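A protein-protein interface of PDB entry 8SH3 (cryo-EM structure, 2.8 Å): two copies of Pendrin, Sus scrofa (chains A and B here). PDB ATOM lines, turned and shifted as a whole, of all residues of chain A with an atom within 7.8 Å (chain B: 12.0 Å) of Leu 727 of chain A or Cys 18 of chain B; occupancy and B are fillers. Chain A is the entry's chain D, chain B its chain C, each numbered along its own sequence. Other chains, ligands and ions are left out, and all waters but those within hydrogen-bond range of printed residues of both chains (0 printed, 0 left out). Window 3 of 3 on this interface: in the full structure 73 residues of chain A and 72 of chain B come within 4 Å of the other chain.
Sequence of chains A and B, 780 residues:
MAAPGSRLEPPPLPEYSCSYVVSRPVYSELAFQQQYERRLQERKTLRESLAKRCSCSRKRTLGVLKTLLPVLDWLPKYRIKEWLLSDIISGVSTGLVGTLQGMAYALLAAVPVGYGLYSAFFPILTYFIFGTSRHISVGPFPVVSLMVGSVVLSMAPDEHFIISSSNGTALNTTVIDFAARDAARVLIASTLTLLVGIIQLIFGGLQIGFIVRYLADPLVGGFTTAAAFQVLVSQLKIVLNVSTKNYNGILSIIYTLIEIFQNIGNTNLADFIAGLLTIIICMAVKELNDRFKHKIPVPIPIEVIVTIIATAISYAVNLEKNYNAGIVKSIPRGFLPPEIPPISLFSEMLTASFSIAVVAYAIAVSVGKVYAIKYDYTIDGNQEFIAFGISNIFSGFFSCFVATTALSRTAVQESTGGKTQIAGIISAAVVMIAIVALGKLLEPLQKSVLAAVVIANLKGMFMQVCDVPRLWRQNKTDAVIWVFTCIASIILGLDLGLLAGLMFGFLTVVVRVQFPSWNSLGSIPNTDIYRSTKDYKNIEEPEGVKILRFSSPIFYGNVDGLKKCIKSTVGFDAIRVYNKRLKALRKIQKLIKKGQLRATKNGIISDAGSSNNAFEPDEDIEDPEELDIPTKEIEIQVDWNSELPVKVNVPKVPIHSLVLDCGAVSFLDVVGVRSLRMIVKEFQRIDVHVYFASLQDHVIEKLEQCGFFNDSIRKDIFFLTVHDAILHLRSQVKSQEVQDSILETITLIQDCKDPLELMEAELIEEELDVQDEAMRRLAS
SG of Cys 18 of chain B sits at hydrogen-bond distance from O of Leu 727 of chain A. N of Tyr 20 of chain B is in hydrogen-bond range of O of Arg 24 of chain A (2.5 Å). OH of Tyr 20 of chain B is in hydrogen-bond range of OD2 of Asp 528 of chain A, at 2.6 Å. The side-chain carboxylate (OD1) of Asp 528 of chain B lies within salt-bridge range of the guanidinium group (NE) of Arg 24 of chain A (3.0 Å).
The backbone NH (N) of Ile 529 of chain B sits at hydrogen-bond distance from the side-chain hydroxyl (OG1) of Thr 527 of chain B (3.2 Å). NH1 of Arg 24 of chain A is in salt-bridge range of OD1 of Asp 724 of chain A. The backbone NH of Tyr 27 of chain A sits at hydrogen-bond distance from the side-chain carboxylate of Asp 724 of chain A. A ring nitrogen (ND1) of His 723 of chain A is in hydrogen-bond range of the side-chain hydroxyl (OH) of Tyr 530 of chain A, 2.9 Å away. The side-chain carboxylate (OD2) of Asp 724 of chain A is in hydrogen-bond range of the side-chain hydroxyl (OG1) of Thr 721 of chain A (3.3 Å).
Arg 24 of chain A touches Thr 527 of chain B. CD of Arg 24 of chain A touches CD1 of Ile 529 of chain B, 3.6 Å away. Val 26 of chain A touches Cys 18 of chain B (N to O, 3.6 Å). CG2 of Val 26 of chain A touches C of Ser 19 of chain B, at 3.7 Å. N of Tyr 20 of chain B touches CG2 of Val 26 of chain A (3.96 Å). CD2 of Tyr 27 of chain A touches CD1 of Ile 529 of chain B (3.7 Å). His 723 of chain A touches Val 22 of chain B. OD1 of Asp 724 of chain A touches CD2 of Tyr 20 of chain B (3.5 Å). O of Ser 19 of chain B touches CD1 of Leu 727 of chain A (3.3 Å). Leu 727 of chain A touches Tyr 20 of chain B.
Of the printed residues of chain B, Arg 24 of chain A touches Ser 19, Tyr 20, Thr 527, Asp 528 and Ile 529. Of chain B, only Cys 18 (3.6 Å), Ser 19 (3.7 Å) and Tyr 20 (3.96 Å) come within 4 Å of Val 26 of chain A. Val 722 of chain A touches none of the printed residues of chain B. Of chain B, only Tyr 20 (3.4 Å) and Val 22 (3.9 Å) come within 4 Å of His 723 of chain A. No residue of chain B comes within 4 Å of Ala 725 of chain A. No residue of chain B comes within 4 Å of Ile 726 of chain A. Of chain B, only Cys 18 (3.6 Å), Ser 19 (3.3 Å) and Tyr 20 (3.8 Å) come within 4 Å of Leu 727 of chain A. No residue of chain B comes within 4 Å of Arg 730 of chain A. No residue of chain B comes within 4 Å of Ser 731 of chain A. Ser 17 of chain B touches none of the printed residues of chain A. Cys 18 of chain B touches just these residues of chain A: Val 26 (3.6 Å) and Leu 727 (3.6 Å). Ser 23 of chain B touches none of the printed residues of chain A. Of the printed residues of chain A, Thr 527 of chain B touches Arg 24 (3.9 Å).
Hydrophobic or aromatic side chains of chain B within 4 Å of the printed part of chain A: Tyr 20, Val 22 and Ile 529. Of the 19 printed residues of chain A, 7 touch a printed residue of chain B. Hydrophobic or aromatic side chains of chain A within 4 Å of the printed part of chain B: Val 26, Tyr 27, His 723 and Leu 727. Among the printed residues, Asp or Glu carboxylates within 4 Å of a Lys or Arg side-chain nitrogen of the other chain: Arg 24 of chain A with Asp 528 of chain B (3.0 Å).
1 position is printed for both chains.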
ATOM      1  N   ARG A  24      -8.298  20.061   0.856  1.00  0.00           N
ATOM      2  CA  ARG A  24      -8.364  18.722   0.291  1.00  0.00           C
ATOM      3  C   ARG A  24      -8.058  17.721   1.395  1.00  0.00           C
ATOM      4  O   ARG A  24      -7.501  18.093   2.433  1.00  0.00           O
ATOM      5  CB  ARG A  24      -7.381  18.566  -0.881  1.00  0.00           C
ATOM      6  CG  ARG A  24      -5.916  18.587  -0.484  1.00  0.00           C
ATOM      7  CD  ARG A  24      -5.076  17.830  -1.497  1.00  0.00           C
ATOM      8  NE  ARG A  24      -3.646  18.059  -1.329  1.00  0.00           N
ATOM      9  CZ  ARG A  24      -2.868  17.365  -0.509  1.00  0.00           C
ATOM     10  NH1 ARG A  24      -3.353  16.396   0.250  1.00  0.00           N
ATOM     11  NH2 ARG A  24      -1.571  17.648  -0.454  1.00  0.00           N
ATOM     12  N   PRO A  25      -8.436  16.460   1.218  1.00  0.00           N
ATOM     13  CA  PRO A  25      -8.078  15.433   2.200  1.00  0.00           C
ATOM     14  C   PRO A  25      -6.575  15.188   2.226  1.00  0.00           C
ATOM     15  O   PRO A  25      -5.853  15.448   1.263  1.00  0.00           O
ATOM     16  CB  PRO A  25      -8.829  14.193   1.702  1.00  0.00           C
ATOM     17  CG  PRO A  25      -9.963  14.741   0.908  1.00  0.00           C
ATOM     18  CD  PRO A  25      -9.400  15.951   0.229  1.00  0.00           C
ATOM     19  N   VAL A  26      -6.109  14.683   3.364  1.00  0.00           N
ATOM     20  CA  VAL A  26      -4.714  14.279   3.511  1.00  0.00           C
ATOM     21  C   VAL A  26      -4.544  12.959   2.767  1.00  0.00           C
ATOM     22  O   VAL A  26      -5.054  11.922   3.196  1.00  0.00           O
ATOM     23  CB  VAL A  26      -4.315  14.145   4.984  1.00  0.00           C
ATOM     24  CG1 VAL A  26      -2.961  13.474   5.105  1.00  0.00           C
ATOM     25  CG2 VAL A  26      -4.293  15.508   5.650  1.00  0.00           C
ATOM     26  N   TYR A  27      -3.832  12.997   1.645  1.00  0.00           N
ATOM     27  CA  TYR A  27      -3.754  11.868   0.729  1.00  0.00           C
ATOM     28  C   TYR A  27      -2.435  11.132   0.913  1.00  0.00           C
ATOM     29  O   TYR A  27      -1.366  11.689   0.646  1.00  0.00           O
ATOM     30  CB  TYR A  27      -3.892  12.333  -0.720  1.00  0.00           C
ATOM     31  CG  TYR A  27      -5.299  12.692  -1.125  1.00  0.00           C
ATOM     32  CD1 TYR A  27      -6.339  11.791  -0.961  1.00  0.00           C
ATOM     33  CD2 TYR A  27      -5.587  13.931  -1.678  1.00  0.00           C
ATOM     34  CE1 TYR A  27      -7.627  12.115  -1.331  1.00  0.00           C
ATOM     35  CE2 TYR A  27      -6.871  14.264  -2.052  1.00  0.00           C
ATOM     36  CZ  TYR A  27      -7.887  13.352  -1.875  1.00  0.00           C
ATOM     37  OH  TYR A  27      -9.170  13.680  -2.248  1.00  0.00           O
ATOM     38  N   ASP A 528       2.945  25.368   4.228  1.00  0.00           N
ATOM     39  CA  ASP A 528       3.346  24.008   3.895  1.00  0.00           C
ATOM     40  C   ASP A 528       4.693  23.974   3.180  1.00  0.00           C
ATOM     41  O   ASP A 528       4.945  23.090   2.359  1.00  0.00           O
ATOM     42  CB  ASP A 528       2.279  23.326   3.040  1.00  0.00           C
ATOM     43  CG  ASP A 528       1.867  24.165   1.849  1.00  0.00           C
ATOM     44  OD1 ASP A 528       2.165  25.377   1.841  1.00  0.00           O
ATOM     45  OD2 ASP A 528       1.251  23.611   0.914  1.00  0.00           O
ATOM     46  N   TYR A 530       8.545  23.413   3.402  1.00  0.00           N
ATOM     47  CA  TYR A 530       9.513  22.744   4.259  1.00  0.00           C
ATOM     48  C   TYR A 530      10.911  23.000   3.716  1.00  0.00           C
ATOM     49  O   TYR A 530      11.255  22.532   2.625  1.00  0.00           O
ATOM     50  CB  TYR A 530       9.211  21.249   4.356  1.00  0.00           C
ATOM     51  CG  TYR A 530       8.016  20.957   5.236  1.00  0.00           C
ATOM     52  CD1 TYR A 530       6.740  21.344   4.852  1.00  0.00           C
ATOM     53  CD2 TYR A 530       8.163  20.317   6.456  1.00  0.00           C
ATOM     54  CE1 TYR A 530       5.645  21.095   5.652  1.00  0.00           C
ATOM     55  CE2 TYR A 530       7.071  20.059   7.261  1.00  0.00           C
ATOM     56  CZ  TYR A 530       5.814  20.450   6.852  1.00  0.00           C
ATOM     57  OH  TYR A 530       4.721  20.201   7.646  1.00  0.00           O
ATOM     58  N   PHE A 719       3.173   9.284   1.250  1.00  0.00           N
ATOM     59  CA  PHE A 719       2.339  10.470   1.147  1.00  0.00           C
ATOM     60  C   PHE A 719       2.747  11.313  -0.055  1.00  0.00           C
ATOM     61  O   PHE A 719       3.855  11.193  -0.582  1.00  0.00           O
ATOM     62  CB  PHE A 719       2.410  11.299   2.432  1.00  0.00           C
ATOM     63  CG  PHE A 719       1.862  10.589   3.635  1.00  0.00           C
ATOM     64  CD1 PHE A 719       0.510  10.638   3.926  1.00  0.00           C
ATOM     65  CD2 PHE A 719       2.695   9.866   4.470  1.00  0.00           C
ATOM     66  CE1 PHE A 719       0.003   9.985   5.029  1.00  0.00           C
ATOM     67  CE2 PHE A 719       2.192   9.211   5.574  1.00  0.00           C
ATOM     68  CZ  PHE A 719       0.845   9.270   5.853  1.00  0.00           C
ATOM     69  N   THR A 721       3.153  14.721  -0.575  1.00  0.00           N
ATOM     70  CA  THR A 721       4.197  15.712  -0.340  1.00  0.00           C
ATOM     71  C   THR A 721       4.590  15.644   1.128  1.00  0.00           C
ATOM     72  O   THR A 721       4.001  14.889   1.906  1.00  0.00           O
ATOM     73  CB  THR A 721       3.731  17.127  -0.710  1.00  0.00           C
ATOM     74  OG1 THR A 721       2.609  17.489   0.103  1.00  0.00           O
ATOM     75  CG2 THR A 721       3.342  17.210  -2.180  1.00  0.00           C
ATOM     76  N   VAL A 722       5.590  16.433   1.524  1.00  0.00           N
ATOM     77  CA  VAL A 722       5.846  16.529   2.954  1.00  0.00           C
ATOM     78  C   VAL A 722       4.989  17.667   3.485  1.00  0.00           C
ATOM     79  O   VAL A 722       5.496  18.729   3.856  1.00  0.00           O
ATOM     80  CB  VAL A 722       7.337  16.783   3.256  1.00  0.00           C
ATOM     81  CG1 VAL A 722       7.609  16.699   4.753  1.00  0.00           C
ATOM     82  CG2 VAL A 722       8.220  15.825   2.484  1.00  0.00           C
ATOM     83  N   HIS A 723       3.683  17.459   3.488  1.00  0.00           N
ATOM     84  CA  HIS A 723       2.743  18.071   4.418  1.00  0.00           C
ATOM     85  C   HIS A 723       1.607  17.138   4.796  1.00  0.00           C
ATOM     86  O   HIS A 723       1.027  17.300   5.873  1.00  0.00           O
ATOM     87  CB  HIS A 723       2.165  19.368   3.839  1.00  0.00           C
ATOM     88  CG  HIS A 723       1.622  20.301   4.876  1.00  0.00           C
ATOM     89  ND1 HIS A 723       2.336  20.664   5.997  1.00  0.00           N
ATOM     90  CD2 HIS A 723       0.435  20.945   4.962  1.00  0.00           C
ATOM     91  CE1 HIS A 723       1.611  21.491   6.729  1.00  0.00           C
ATOM     92  NE2 HIS A 723       0.452  21.678   6.123  1.00  0.00           N
ATOM     93  N   ASP A 724       1.273  16.164   3.944  1.00  0.00           N
ATOM     94  CA  ASP A 724       0.303  15.139   4.297  1.00  0.00           C
ATOM     95  C   ASP A 724       0.851  14.235   5.388  1.00  0.00           C
ATOM     96  O   ASP A 724       0.109  13.808   6.280  1.00  0.00           O
ATOM     97  CB  ASP A 724      -0.059  14.319   3.058  1.00  0.00           C
ATOM     98  CG  ASP A 724      -0.659  15.165   1.952  1.00  0.00           C
ATOM     99  OD1 ASP A 724      -1.869  15.462   2.014  1.00  0.00           O
ATOM    100  OD2 ASP A 724       0.082  15.531   1.017  1.00  0.00           O
ATOM    101  N   ALA A 725       2.148  13.926   5.328  1.00  0.00           N
ATOM    102  CA  ALA A 725       2.766  13.109   6.364  1.00  0.00           C
ATOM    103  C   ALA A 725       2.711  13.801   7.718  1.00  0.00           C
ATOM    104  O   ALA A 725       2.340  13.185   8.721  1.00  0.00           O
ATOM    105  CB  ALA A 725       4.209  12.786   5.982  1.00  0.00           C
ATOM    106  N   ILE A 726       3.059  15.088   7.765  1.00  0.00           N
ATOM    107  CA  ILE A 726       3.069  15.806   9.035  1.00  0.00           C
ATOM    108  C   ILE A 726       1.656  15.959   9.581  1.00  0.00           C
ATOM    109  O   ILE A 726       1.424  15.823  10.788  1.00  0.00           O
ATOM    110  CB  ILE A 726       3.768  17.166   8.870  1.00  0.00           C
ATOM    111  CG1 ILE A 726       5.112  16.978   8.168  1.00  0.00           C
ATOM    112  CG2 ILE A 726       3.965  17.829  10.219  1.00  0.00           C
ATOM    113  CD1 ILE A 726       6.058  16.083   8.923  1.00  0.00           C
ATOM    114  N   LEU A 727       0.690  16.249   8.709  1.00  0.00           N
ATOM    115  CA  LEU A 727      -0.695  16.369   9.153  1.00  0.00           C
ATOM    116  C   LEU A 727      -1.233  15.031   9.645  1.00  0.00           C
ATOM    117  O   LEU A 727      -2.011  14.982  10.605  1.00  0.00           O
ATOM    118  CB  LEU A 727      -1.560  16.917   8.020  1.00  0.00           C
ATOM    119  CG  LEU A 727      -1.409  18.412   7.736  1.00  0.00           C
ATOM    120  CD1 LEU A 727      -2.435  18.870   6.716  1.00  0.00           C
ATOM    121  CD2 LEU A 727      -1.527  19.216   9.019  1.00  0.00           C
ATOM    122  N   HIS A 728      -0.839  13.936   8.991  1.00  0.00           N
ATOM    123  CA  HIS A 728      -1.229  12.608   9.449  1.00  0.00           C
ATOM    124  C   HIS A 728      -0.622  12.295  10.810  1.00  0.00           C
ATOM    125  O   HIS A 728      -1.285  11.713  11.677  1.00  0.00           O
ATOM    126  CB  HIS A 728      -0.808  11.567   8.411  1.00  0.00           C
ATOM    127  CG  HIS A 728      -1.064  10.153   8.827  1.00  0.00           C
ATOM    128  ND1 HIS A 728      -2.308   9.565   8.741  1.00  0.00           N
ATOM    129  CD2 HIS A 728      -0.233   9.204   9.321  1.00  0.00           C
ATOM    130  CE1 HIS A 728      -2.234   8.319   9.170  1.00  0.00           C
ATOM    131  NE2 HIS A 728      -0.986   8.074   9.527  1.00  0.00           N
ATOM    132  N   LEU A 729       0.642  12.669  11.014  1.00  0.00           N
ATOM    133  CA  LEU A 729       1.283  12.480  12.312  1.00  0.00           C
ATOM    134  C   LEU A 729       0.589  13.286  13.402  1.00  0.00           C
ATOM    135  O   LEU A 729       0.383  12.785  14.513  1.00  0.00           O
ATOM    136  CB  LEU A 729       2.757  12.863  12.228  1.00  0.00           C
ATOM    137  CG  LEU A 729       3.776  11.765  11.938  1.00  0.00           C
ATOM    138  CD1 LEU A 729       3.541  11.128  10.591  1.00  0.00           C
ATOM    139  CD2 LEU A 729       5.157  12.376  11.990  1.00  0.00           C
ATOM    140  N   ARG A 730       0.232  14.537  13.108  1.00  0.00           N
ATOM    141  CA  ARG A 730      -0.463  15.356  14.093  1.00  0.00           C
ATOM    142  C   ARG A 730      -1.839  14.799  14.432  1.00  0.00           C
ATOM    143  O   ARG A 730      -2.367  15.094  15.509  1.00  0.00           O
ATOM    144  CB  ARG A 730      -0.587  16.794  13.591  1.00  0.00           C
ATOM    145  CG  ARG A 730       0.741  17.526  13.489  1.00  0.00           C
ATOM    146  CD  ARG A 730       0.539  19.008  13.233  1.00  0.00           C
ATOM    147  NE  ARG A 730       1.621  19.572  12.433  1.00  0.00           N
ATOM    148  CZ  ARG A 730       1.478  20.582  11.587  1.00  0.00           C
ATOM    149  NH1 ARG A 730       0.308  21.171  11.406  1.00  0.00           N
ATOM    150  NH2 ARG A 730       2.536  21.012  10.906  1.00  0.00           N
ATOM    151  N   SER A 731      -2.429  14.002  13.539  1.00  0.00           N
ATOM    152  CA  SER A 731      -3.705  13.360  13.822  1.00  0.00           C
ATOM    153  C   SER A 731      -3.583  12.223  14.826  1.00  0.00           C
ATOM    154  O   SER A 731      -4.608  11.757  15.335  1.00  0.00           O
ATOM    155  CB  SER A 731      -4.328  12.840  12.525  1.00  0.00           C
ATOM    156  OG  SER A 731      -5.433  11.996  12.793  1.00  0.00           O
ATOM    157  N   GLN A 732      -2.369  11.767  15.119  1.00  0.00           N
ATOM    158  CA  GLN A 732      -2.159  10.708  16.099  1.00  0.00           C
ATOM    159  C   GLN A 732      -1.468  11.249  17.345  1.00  0.00           C
ATOM    160  O   GLN A 732      -2.023  12.080  18.064  1.00  0.00           O
ATOM    161  CB  GLN A 732      -1.335   9.570  15.493  1.00  0.00           C
ATOM    162  CG  GLN A 732      -1.823   9.105  14.132  1.00  0.00           C
ATOM    163  CD  GLN A 732      -0.759   8.348  13.362  1.00  0.00           C
ATOM    164  OE1 GLN A 732       0.436   8.539  13.582  1.00  0.00           O
ATOM    165  NE2 GLN A 732      -1.191   7.477  12.459  1.00  0.00           N
ATOM    166  N   SER B  17     -11.644  12.482   7.549  1.00  0.00           N
ATOM    167  CA  SER B  17     -10.867  12.637   8.774  1.00  0.00           C
ATOM    168  C   SER B  17     -10.041  13.918   8.737  1.00  0.00           C
ATOM    169  O   SER B  17     -10.590  15.020   8.708  1.00  0.00           O
ATOM    170  CB  SER B  17      -9.955  11.428   8.989  1.00  0.00           C
ATOM    171  OG  SER B  17      -9.261  11.526  10.220  1.00  0.00           O
ATOM    172  N   CYS B  18      -8.718  13.766   8.742  1.00  0.00           N
ATOM    173  CA  CYS B  18      -7.833  14.918   8.686  1.00  0.00           C
ATOM    174  C   CYS B  18      -7.923  15.594   7.323  1.00  0.00           C
ATOM    175  O   CYS B  18      -8.202  14.957   6.304  1.00  0.00           O
ATOM    176  CB  CYS B  18      -6.391  14.499   8.973  1.00  0.00           C
ATOM    177  SG  CYS B  18      -5.233  15.876   9.149  1.00  0.00           S
ATOM    178  N   SER B  19      -7.682  16.903   7.312  1.00  0.00           N
ATOM    179  CA  SER B  19      -7.813  17.708   6.109  1.00  0.00           C
ATOM    180  C   SER B  19      -6.519  18.460   5.837  1.00  0.00           C
ATOM    181  O   SER B  19      -5.748  18.761   6.752  1.00  0.00           O
ATOM    182  CB  SER B  19      -8.975  18.702   6.224  1.00  0.00           C
ATOM    183  OG  SER B  19      -8.724  19.665   7.231  1.00  0.00           O
ATOM    184  N   TYR B  20      -6.291  18.755   4.561  1.00  0.00           N
ATOM    185  CA  TYR B  20      -5.134  19.522   4.106  1.00  0.00           C
ATOM    186  C   TYR B  20      -5.614  20.938   3.811  1.00  0.00           C
ATOM    187  O   TYR B  20      -6.108  21.224   2.717  1.00  0.00           O
ATOM    188  CB  TYR B  20      -4.508  18.864   2.880  1.00  0.00           C
ATOM    189  CG  TYR B  20      -3.223  19.491   2.390  1.00  0.00           C
ATOM    190  CD1 TYR B  20      -3.235  20.653   1.632  1.00  0.00           C
ATOM    191  CD2 TYR B  20      -1.998  18.904   2.667  1.00  0.00           C
ATOM    192  CE1 TYR B  20      -2.063  21.221   1.177  1.00  0.00           C
ATOM    193  CE2 TYR B  20      -0.824  19.464   2.214  1.00  0.00           C
ATOM    194  CZ  TYR B  20      -0.860  20.621   1.472  1.00  0.00           C
ATOM    195  OH  TYR B  20       0.313  21.180   1.021  1.00  0.00           O
ATOM    196  N   VAL B  21      -5.473  21.825   4.791  1.00  0.00           N
ATOM    197  CA  VAL B  21      -5.907  23.213   4.674  1.00  0.00           C
ATOM    198  C   VAL B  21      -4.683  24.104   4.826  1.00  0.00           C
ATOM    199  O   VAL B  21      -4.045  24.116   5.887  1.00  0.00           O
ATOM    200  CB  VAL B  21      -6.977  23.567   5.719  1.00  0.00           C
ATOM    201  CG1 VAL B  21      -7.399  25.017   5.572  1.00  0.00           C
ATOM    202  CG2 VAL B  21      -8.172  22.642   5.584  1.00  0.00           C
ATOM    203  N   VAL B  22      -4.355  24.844   3.770  1.00  0.00           N
ATOM    204  CA  VAL B  22      -3.225  25.764   3.765  1.00  0.00           C
ATOM    205  C   VAL B  22      -3.698  27.109   3.232  1.00  0.00           C
ATOM    206  O   VAL B  22      -4.318  27.176   2.166  1.00  0.00           O
ATOM    207  CB  VAL B  22      -2.052  25.235   2.917  1.00  0.00           C
ATOM    208  CG1 VAL B  22      -0.902  26.228   2.930  1.00  0.00           C
ATOM    209  CG2 VAL B  22      -1.588  23.885   3.434  1.00  0.00           C
ATOM    210  N   SER B  23      -3.408  28.174   3.975  1.00  0.00           N
ATOM    211  CA  SER B  23      -3.683  29.540   3.550  1.00  0.00           C
ATOM    212  C   SER B  23      -2.399  30.344   3.684  1.00  0.00           C
ATOM    213  O   SER B  23      -1.927  30.581   4.801  1.00  0.00           O
ATOM    214  CB  SER B  23      -4.806  30.165   4.379  1.00  0.00           C
ATOM    215  OG  SER B  23      -5.100  31.475   3.930  1.00  0.00           O
ATOM    216  N   THR B 527      -7.675  20.612  -6.052  1.00  0.00           N
ATOM    217  CA  THR B 527      -6.520  20.319  -5.214  1.00  0.00           C
ATOM    218  C   THR B 527      -5.277  20.943  -5.839  1.00  0.00           C
ATOM    219  O   THR B 527      -5.341  21.617  -6.871  1.00  0.00           O
ATOM    220  CB  THR B 527      -6.311  18.809  -5.026  1.00  0.00           C
ATOM    221  OG1 THR B 527      -5.647  18.271  -6.175  1.00  0.00           O
ATOM    222  CG2 THR B 527      -7.637  18.087  -4.826  1.00  0.00           C
ATOM    223  N   ASP B 528      -4.131  20.713  -5.197  1.00  0.00           N
ATOM    224  CA  ASP B 528      -2.841  21.181  -5.685  1.00  0.00           C
ATOM    225  C   ASP B 528      -1.923  20.021  -6.057  1.00  0.00           C
ATOM    226  O   ASP B 528      -0.700  20.128  -5.946  1.00  0.00           O
ATOM    227  CB  ASP B 528      -2.165  22.073  -4.646  1.00  0.00           C
ATOM    228  CG  ASP B 528      -2.092  21.423  -3.280  1.00  0.00           C
ATOM    229  OD1 ASP B 528      -2.826  20.440  -3.049  1.00  0.00           O
ATOM    230  OD2 ASP B 528      -1.297  21.890  -2.439  1.00  0.00           O
ATOM    231  N   ILE B 529      -2.499  18.908  -6.498  1.00  0.00           N
ATOM    232  CA  ILE B 529      -1.751  17.702  -6.829  1.00  0.00           C
ATOM    233  C   ILE B 529      -1.645  17.631  -8.344  1.00  0.00           C
ATOM    234  O   ILE B 529      -2.646  17.439  -9.039  1.00  0.00           O
ATOM    235  CB  ILE B 529      -2.426  16.448  -6.262  1.00  0.00           C
ATOM    236  CG1 ILE B 529      -2.730  16.635  -4.774  1.00  0.00           C
ATOM    237  CG2 ILE B 529      -1.553  15.223  -6.490  1.00  0.00           C
ATOM    238  CD1 ILE B 529      -3.936  15.862  -4.304  1.00  0.00           C
